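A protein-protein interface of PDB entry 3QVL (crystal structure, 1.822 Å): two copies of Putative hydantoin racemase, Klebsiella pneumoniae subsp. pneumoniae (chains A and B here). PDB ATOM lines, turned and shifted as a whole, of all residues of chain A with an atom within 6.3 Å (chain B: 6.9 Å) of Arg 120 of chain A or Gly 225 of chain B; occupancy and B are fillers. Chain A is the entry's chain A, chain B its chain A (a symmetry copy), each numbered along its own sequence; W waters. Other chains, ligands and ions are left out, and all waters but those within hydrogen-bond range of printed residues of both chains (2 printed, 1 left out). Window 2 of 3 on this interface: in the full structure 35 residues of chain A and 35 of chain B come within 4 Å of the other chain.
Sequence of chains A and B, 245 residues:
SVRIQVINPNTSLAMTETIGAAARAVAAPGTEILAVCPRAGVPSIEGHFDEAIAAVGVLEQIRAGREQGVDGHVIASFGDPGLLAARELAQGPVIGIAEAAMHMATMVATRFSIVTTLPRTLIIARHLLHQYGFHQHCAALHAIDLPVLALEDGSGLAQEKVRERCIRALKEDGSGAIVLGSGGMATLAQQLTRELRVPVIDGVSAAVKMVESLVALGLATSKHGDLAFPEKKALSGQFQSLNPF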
ATOM      1  N   GLU A  46      -7.991  -8.715 -30.068  1.00  0.00           N
ATOM      2  CA  GLU A  46      -8.215  -7.822 -28.933  1.00  0.00           C
ATOM      3  C   GLU A  46      -7.944  -6.364 -29.299  1.00  0.00           C
ATOM      4  O   GLU A  46      -7.237  -5.653 -28.581  1.00  0.00           O
ATOM      5  CB  GLU A  46      -7.331  -8.238 -27.753  1.00  0.00           C
ATOM      6  CG  GLU A  46      -7.608  -9.638 -27.219  1.00  0.00           C
ATOM      7  CD  GLU A  46      -6.629 -10.068 -26.144  1.00  0.00           C
ATOM      8  OE1 GLU A  46      -5.408  -9.870 -26.326  1.00  0.00           O
ATOM      9  OE2 GLU A  46      -7.082 -10.617 -25.118  1.00  0.00           O
ATOM     10  N   GLY A  47      -8.507  -5.927 -30.420  1.00  0.00           N
ATOM     11  CA  GLY A  47      -8.321  -4.559 -30.890  1.00  0.00           C
ATOM     12  C   GLY A  47      -8.322  -4.446 -32.401  1.00  0.00           C
ATOM     13  O   GLY A  47      -8.506  -5.440 -33.108  1.00  0.00           O
ATOM     14  N   HIS A  48      -8.100  -3.229 -32.887  1.00  0.00           N
ATOM     15  CA  HIS A  48      -8.203  -2.913 -34.311  1.00  0.00           C
ATOM     16  C   HIS A  48      -7.037  -3.476 -35.126  1.00  0.00           C
ATOM     17  O   HIS A  48      -7.224  -3.916 -36.263  1.00  0.00           O
ATOM     18  CB  HIS A  48      -8.327  -1.399 -34.510  1.00  0.00           C
ATOM     19  CG  HIS A  48      -9.350  -0.757 -33.623  1.00  0.00           C
ATOM     20  ND1 HIS A  48     -10.671  -0.614 -33.990  1.00  0.00           N
ATOM     21  CD2 HIS A  48      -9.246  -0.227 -32.382  1.00  0.00           C
ATOM     22  CE1 HIS A  48     -11.336  -0.024 -33.013  1.00  0.00           C
ATOM     23  NE2 HIS A  48     -10.494   0.222 -32.025  1.00  0.00           N
ATOM     24  N   LEU A 118     -12.877  -8.479 -23.291  1.00  0.00           N
ATOM     25  CA  LEU A 118     -11.995  -7.340 -22.995  1.00  0.00           C
ATOM     26  C   LEU A 118     -12.679  -5.987 -23.206  1.00  0.00           C
ATOM     27  O   LEU A 118     -13.367  -5.798 -24.211  1.00  0.00           O
ATOM     28  CB  LEU A 118     -10.719  -7.391 -23.846  1.00  0.00           C
ATOM     29  CG  LEU A 118      -9.381  -7.897 -23.291  1.00  0.00           C
ATOM     30  CD1 LEU A 118      -8.272  -7.480 -24.239  1.00  0.00           C
ATOM     31  CD2 LEU A 118      -9.075  -7.382 -21.890  1.00  0.00           C
ATOM     32  N   PRO A 119     -12.478  -5.040 -22.264  1.00  0.00           N
ATOM     33  CA  PRO A 119     -13.031  -3.682 -22.355  1.00  0.00           C
ATOM     34  C   PRO A 119     -12.686  -2.921 -23.639  1.00  0.00           C
ATOM     35  O   PRO A 119     -13.536  -2.200 -24.162  1.00  0.00           O
ATOM     36  CB  PRO A 119     -12.415  -2.976 -21.143  1.00  0.00           C
ATOM     37  CG  PRO A 119     -12.221  -4.059 -20.156  1.00  0.00           C
ATOM     38  CD  PRO A 119     -11.827  -5.267 -20.958  1.00  0.00           C
ATOM     39  N   ARG A 120     -11.462  -3.078 -24.143  1.00  0.00           N
ATOM     40  CA  ARG A 120     -11.028  -2.339 -25.336  1.00  0.00           C
ATOM     41  C   ARG A 120     -11.711  -2.805 -26.631  1.00  0.00           C
ATOM     42  O   ARG A 120     -11.599  -2.145 -27.668  1.00  0.00           O
ATOM     43  CB  ARG A 120      -9.498  -2.351 -25.477  1.00  0.00           C
ATOM     44  CG  ARG A 120      -8.884  -3.694 -25.856  1.00  0.00           C
ATOM     45  CD  ARG A 120      -7.380  -3.568 -26.070  1.00  0.00           C
ATOM     46  NE  ARG A 120      -7.049  -2.676 -27.183  1.00  0.00           N
ATOM     47  CZ  ARG A 120      -5.815  -2.291 -27.502  1.00  0.00           C
ATOM     48  NH1 ARG A 120      -4.770  -2.715 -26.802  1.00  0.00           N
ATOM     49  NH2 ARG A 120      -5.624  -1.475 -28.530  1.00  0.00           N
ATOM     50  N   THR A 121     -12.417  -3.933 -26.562  1.00  0.00           N
ATOM     51  CA  THR A 121     -13.163  -4.455 -27.708  1.00  0.00           C
ATOM     52  C   THR A 121     -14.609  -3.951 -27.737  1.00  0.00           C
ATOM     53  O   THR A 121     -15.328  -4.179 -28.712  1.00  0.00           O
ATOM     54  CB  THR A 121     -13.152  -6.005 -27.764  1.00  0.00           C
ATOM     55  OG1 THR A 121     -13.915  -6.538 -26.676  1.00  0.00           O
ATOM     56  CG2 THR A 121     -11.726  -6.547 -27.709  1.00  0.00           C
ATOM     57  N   LEU A 122     -15.030  -3.270 -26.670  1.00  0.00           N
ATOM     58  CA  LEU A 122     -16.388  -2.723 -26.588  1.00  0.00           C
ATOM     59  C   LEU A 122     -16.669  -1.711 -27.699  1.00  0.00           C
ATOM     60  O   LEU A 122     -17.770  -1.686 -28.251  1.00  0.00           O
ATOM     61  CB  LEU A 122     -16.655  -2.100 -25.211  1.00  0.00           C
ATOM     62  CG  LEU A 122     -16.844  -3.047 -24.019  1.00  0.00           C
ATOM     63  CD1 LEU A 122     -16.654  -2.301 -22.707  1.00  0.00           C
ATOM     64  CD2 LEU A 122     -18.205  -3.732 -24.054  1.00  0.00           C
ATOM     65  N   ILE A 123     -15.665  -0.898 -28.030  1.00  0.00           N
ATOM     66  CA  ILE A 123     -15.771   0.087 -29.112  1.00  0.00           C
ATOM     67  C   ILE A 123     -16.014  -0.575 -30.476  1.00  0.00           C
ATOM     68  O   ILE A 123     -16.748  -0.039 -31.310  1.00  0.00           O
ATOM     69  CB  ILE A 123     -14.536   1.051 -29.153  1.00  0.00           C
ATOM     70  CG1 ILE A 123     -14.800   2.266 -30.054  1.00  0.00           C
ATOM     71  CG2 ILE A 123     -13.253   0.319 -29.564  1.00  0.00           C
ATOM     72  CD1 ILE A 123     -15.771   3.283 -29.472  1.00  0.00           C
ATOM     73  N   ILE A 124     -15.403  -1.741 -30.685  1.00  0.00           N
ATOM     74  CA  ILE A 124     -15.587  -2.522 -31.910  1.00  0.00           C
ATOM     75  C   ILE A 124     -17.033  -3.017 -32.013  1.00  0.00           C
ATOM     76  O   ILE A 124     -17.640  -2.960 -33.086  1.00  0.00           O
ATOM     77  CB  ILE A 124     -14.581  -3.706 -31.991  1.00  0.00           C
ATOM     78  CG1 ILE A 124     -13.139  -3.180 -32.024  1.00  0.00           C
ATOM     79  CG2 ILE A 124     -14.862  -4.589 -33.212  1.00  0.00           C
ATOM     80  CD1 ILE A 124     -12.069  -4.238 -31.787  1.00  0.00           C
ATOM     81  N   ALA A 143     -18.161  -5.847 -20.509  1.00  0.00           N
ATOM     82  CA  ALA A 143     -16.994  -6.712 -20.629  1.00  0.00           C
ATOM     83  C   ALA A 143     -16.671  -7.324 -19.270  1.00  0.00           C
ATOM     84  O   ALA A 143     -16.824  -6.665 -18.238  1.00  0.00           O
ATOM     85  CB  ALA A 143     -15.806  -5.933 -21.161  1.00  0.00           C
ATOM     86  N   GLU B  88      -3.389   2.368 -33.241  1.00  0.00           N
ATOM     87  CA  GLU B  88      -2.937   1.480 -32.172  1.00  0.00           C
ATOM     88  C   GLU B  88      -1.432   1.236 -32.255  1.00  0.00           C
ATOM     89  O   GLU B  88      -0.730   1.321 -31.245  1.00  0.00           O
ATOM     90  CB  GLU B  88      -3.680   0.143 -32.222  1.00  0.00           C
ATOM     91  CG  GLU B  88      -5.132   0.207 -31.771  1.00  0.00           C
ATOM     92  CD  GLU B  88      -5.786  -1.163 -31.688  1.00  0.00           C
ATOM     93  OE1 GLU B  88      -5.167  -2.159 -32.113  1.00  0.00           O
ATOM     94  OE2 GLU B  88      -6.924  -1.246 -31.187  1.00  0.00           O
ATOM     95  N   SER B 222      -4.178   8.850 -28.216  1.00  0.00           N
ATOM     96  CA  SER B 222      -4.372   8.402 -26.843  1.00  0.00           C
ATOM     97  C   SER B 222      -4.032   6.925 -26.716  1.00  0.00           C
ATOM     98  O   SER B 222      -4.539   6.095 -27.475  1.00  0.00           O
ATOM     99  CB  SER B 222      -5.816   8.632 -26.400  1.00  0.00           C
ATOM    100  OG  SER B 222      -6.003   8.209 -25.059  1.00  0.00           O
ATOM    101  N   LYS B 223      -3.167   6.609 -25.758  1.00  0.00           N
ATOM    102  CA  LYS B 223      -2.817   5.223 -25.461  1.00  0.00           C
ATOM    103  C   LYS B 223      -3.589   4.717 -24.244  1.00  0.00           C
ATOM    104  O   LYS B 223      -3.253   3.687 -23.654  1.00  0.00           O
ATOM    105  CB  LYS B 223      -1.302   5.070 -25.277  1.00  0.00           C
ATOM    106  CG  LYS B 223      -0.497   5.305 -26.552  1.00  0.00           C
ATOM    107  CD  LYS B 223      -0.848   4.283 -27.631  1.00  0.00           C
ATOM    108  CE  LYS B 223      -0.489   4.788 -29.012  1.00  0.00           C
ATOM    109  NZ  LYS B 223      -0.977   3.862 -30.072  1.00  0.00           N
ATOM    110  N   HIS B 224      -4.632   5.461 -23.884  1.00  0.00           N
ATOM    111  CA  HIS B 224      -5.546   5.083 -22.817  1.00  0.00           C
ATOM    112  C   HIS B 224      -6.788   4.428 -23.415  1.00  0.00           C
ATOM    113  O   HIS B 224      -7.647   5.104 -23.989  1.00  0.00           O
ATOM    114  CB  HIS B 224      -5.925   6.316 -21.990  1.00  0.00           C
ATOM    115  CG  HIS B 224      -6.984   6.062 -20.962  1.00  0.00           C
ATOM    116  ND1 HIS B 224      -6.712   5.482 -19.742  1.00  0.00           N
ATOM    117  CD2 HIS B 224      -8.312   6.323 -20.968  1.00  0.00           C
ATOM    118  CE1 HIS B 224      -7.830   5.388 -19.043  1.00  0.00           C
ATOM    119  NE2 HIS B 224      -8.815   5.892 -19.763  1.00  0.00           N
ATOM    120  N   GLY B 225      -6.862   3.106 -23.294  1.00  0.00           N
ATOM    121  CA  GLY B 225      -8.046   2.353 -23.696  1.00  0.00           C
ATOM    122  C   GLY B 225      -8.055   1.827 -25.120  1.00  0.00           C
ATOM    123  O   GLY B 225      -7.265   0.948 -25.474  1.00  0.00           O
ATOM    124  N   ASP B 226      -8.953   2.380 -25.932  1.00  0.00           N
ATOM    125  CA  ASP B 226      -9.289   1.834 -27.252  1.00  0.00           C
ATOM    126  C   ASP B 226      -8.154   1.827 -28.274  1.00  0.00           C
ATOM    127  O   ASP B 226      -8.066   0.915 -29.098  1.00  0.00           O
ATOM    128  CB  ASP B 226     -10.500   2.569 -27.839  1.00  0.00           C
ATOM    129  CG  ASP B 226     -11.762   2.380 -27.014  1.00  0.00           C
ATOM    130  OD1 ASP B 226     -11.771   1.529 -26.099  1.00  0.00           O
ATOM    131  OD2 ASP B 226     -12.753   3.087 -27.289  1.00  0.00           O
ATOM    132  N   LEU B 227      -7.298   2.845 -28.225  1.00  0.00           N
ATOM    133  CA  LEU B 227      -6.221   2.982 -29.202  1.00  0.00           C
ATOM    134  C   LEU B 227      -4.838   2.778 -28.582  1.00  0.00           C
ATOM    135  O   LEU B 227      -3.827   3.235 -29.122  1.00  0.00           O
ATOM    136  CB  LEU B 227      -6.313   4.330 -29.928  1.00  0.00           C
ATOM    137  CG  LEU B 227      -7.588   4.621 -30.732  1.00  0.00           C
ATOM    138  CD1 LEU B 227      -7.564   6.041 -31.270  1.00  0.00           C
ATOM    139  CD2 LEU B 227      -7.792   3.620 -31.868  1.00  0.00           C
ATOM    140  N   ALA B 228      -4.810   2.074 -27.452  1.00  0.00           N
ATOM    141  CA  ALA B 228      -3.562   1.664 -26.817  1.00  0.00           C
ATOM    142  C   ALA B 228      -2.787   0.746 -27.757  1.00  0.00           C
ATOM    143  O   ALA B 228      -3.367   0.157 -28.676  1.00  0.00           O
ATOM    144  CB  ALA B 228      -3.852   0.950 -25.504  1.00  0.00           C
ATOM    145  N   PHE B 229      -1.480   0.635 -27.535  1.00  0.00           N
ATOM    146  CA  PHE B 229      -0.652  -0.291 -28.304  1.00  0.00           C
ATOM    147  C   PHE B 229      -1.259  -1.694 -28.247  1.00  0.00           C
ATOM    148  O   PHE B 229      -1.832  -2.074 -27.223  1.00  0.00           O
ATOM    149  CB  PHE B 229       0.789  -0.303 -27.784  1.00  0.00           C
ATOM    150  CG  PHE B 229       1.515   1.001 -27.969  1.00  0.00           C
ATOM    151  CD1 PHE B 229       1.857   1.454 -29.242  1.00  0.00           C
ATOM    152  CD2 PHE B 229       1.870   1.774 -26.868  1.00  0.00           C
ATOM    153  CE1 PHE B 229       2.532   2.661 -29.416  1.00  0.00           C
ATOM    154  CE2 PHE B 229       2.549   2.982 -27.031  1.00  0.00           C
ATOM    155  CZ  PHE B 229       2.879   3.426 -28.306  1.00  0.00           C
ATOM    156  N   PRO B 230      -1.152  -2.460 -29.349  1.00  0.00           N
ATOM    157  CA  PRO B 230      -1.733  -3.803 -29.385  1.00  0.00           C
ATOM    158  C   PRO B 230      -1.247  -4.660 -28.220  1.00  0.00           C
ATOM    159  O   PRO B 230      -0.097  -4.523 -27.792  1.00  0.00           O
ATOM    160  CB  PRO B 230      -1.216  -4.372 -30.707  1.00  0.00           C
ATOM    161  CG  PRO B 230      -0.947  -3.184 -31.550  1.00  0.00           C
ATOM    162  CD  PRO B 230      -0.478  -2.120 -30.615  1.00  0.00           C
ATOM    163  N   GLU B 231      -2.122  -5.521 -27.707  1.00  0.00           N
ATOM    164  CA  GLU B 231      -1.762  -6.440 -26.629  1.00  0.00           C
ATOM    165  C   GLU B 231      -0.604  -7.328 -27.076  1.00  0.00           C
ATOM    166  O   GLU B 231      -0.568  -7.774 -28.225  1.00  0.00           O
ATOM    167  CB  GLU B 231      -2.961  -7.300 -26.212  1.00  0.00           C
ATOM    168  CG  GLU B 231      -4.206  -6.515 -25.785  1.00  0.00           C
ATOM    169  CD  GLU B 231      -3.982  -5.642 -24.557  1.00  0.00           C
ATOM    170  OE1 GLU B 231      -3.293  -6.086 -23.612  1.00  0.00           O
ATOM    171  OE2 GLU B 231      -4.506  -4.509 -24.536  1.00  0.00           O
HETATM  172  O   HOH W   1     -13.992   0.000 -25.704  1.00  0.00           O
HETATM  173  O   HOH W   2      -4.514  -6.104 -29.240  1.00  0.00           O
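Water W1 lies within hydrogen-bond range of O of Pro 119 of chain A (2.7 Å), OD1 of Asp 226 of chain B (2.7 Å) and N of Ile 123 of chain A (3.0 Å). Water W2 bridges the backbone carbonyl oxygen of Glu 46 of chain A (2.8 Å) and the backbone NH of Glu 231 of chain B (2.9 Å).
Of the printed residues of chain B, Arg 120 of chain A touches Glu 88 (3.0 Å), Gly 225 (3.98 Å), Asp 226 (3.5 Å), Ala 228 (2.8 Å), Phe 229 (3.0 Å) and Glu 231 (2.9 Å). Of the printed residues of chain B, Ile 123 of chain A touches Asp 226 (3.3 Å). Of the printed residues of chain A, Gly 225 of chain B touches Arg 120. Of the printed residues of chain A, Phe 229 of chain B touches Arg 120.
Glu 46 of chain A touches Glu 231 of chain B (OE1 to CB, 3.6 Å). Glu 88 of chain B touches Gly 47 of chain A. Asp 226 of chain B touches His 48 of chain A (O to CD2, 3.7 Å). CB of Arg 120 of chain A touches O of Gly 225 of chain B (3.98 Å). OD2 of Asp 226 of chain B touches CB of Ile 123 of chain A, at 3.3 Å.
Of the 11 printed residues of chain B, 6 touch a printed residue of chain A. Printed residues of chain B that touch a printed residue of chain A: Glu 88, Gly 225, Asp 226, Ala 228, Phe 229 and Glu 231. Along chain A the printed residues that touch a printed residue of chain B span positions 46 to 123. Among the printed residues, 11 pairs touch across the chains. Among the printed residues, Asp or Glu carboxylates within 4 Å of a Lys or Arg side-chain nitrogen of the other chain: Arg 120 of chain A with Glu 88 of chain B (3.0 Å) and Arg 120 of chain A with Glu 231 of chain B (2.9 Å).
O of Glu 46 of chain A sits close to NE of Arg 120 of chain A, 3.3 Å away. The backbone carbonyl oxygen (O) of Glu 88 of chain B is in hydrogen-bond range of the side-chain amino group (NZ) of Lys 223 of chain B.
No position is printed for both chains.
N of His 48 of chain A lies close to OE2 of Glu 88 of chain B, at 2.9 Å. The guanidinium group (NH2) of Arg 120 of chain A is in salt-bridge range of the side-chain carboxylate (OE2) of Glu 88 of chain B (3.0 Å). The guanidinium group of Arg 120 of chain A sits at hydrogen-bond distance from the backbone carbonyl oxygen of Asp 226 of chain B (3.5 Å). O of Ala 228 of chain B lies within hydrogen-bond range of NH2 of Arg 120 of chain A (2.8 Å). NH1 of Arg 120 of chain A sits at hydrogen-bond distance from O of Phe 229 of chain B. NH1 of Arg 120 of chain A is in salt-bridge range of OE2 of Glu 231 of chain B (2.9 Å).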
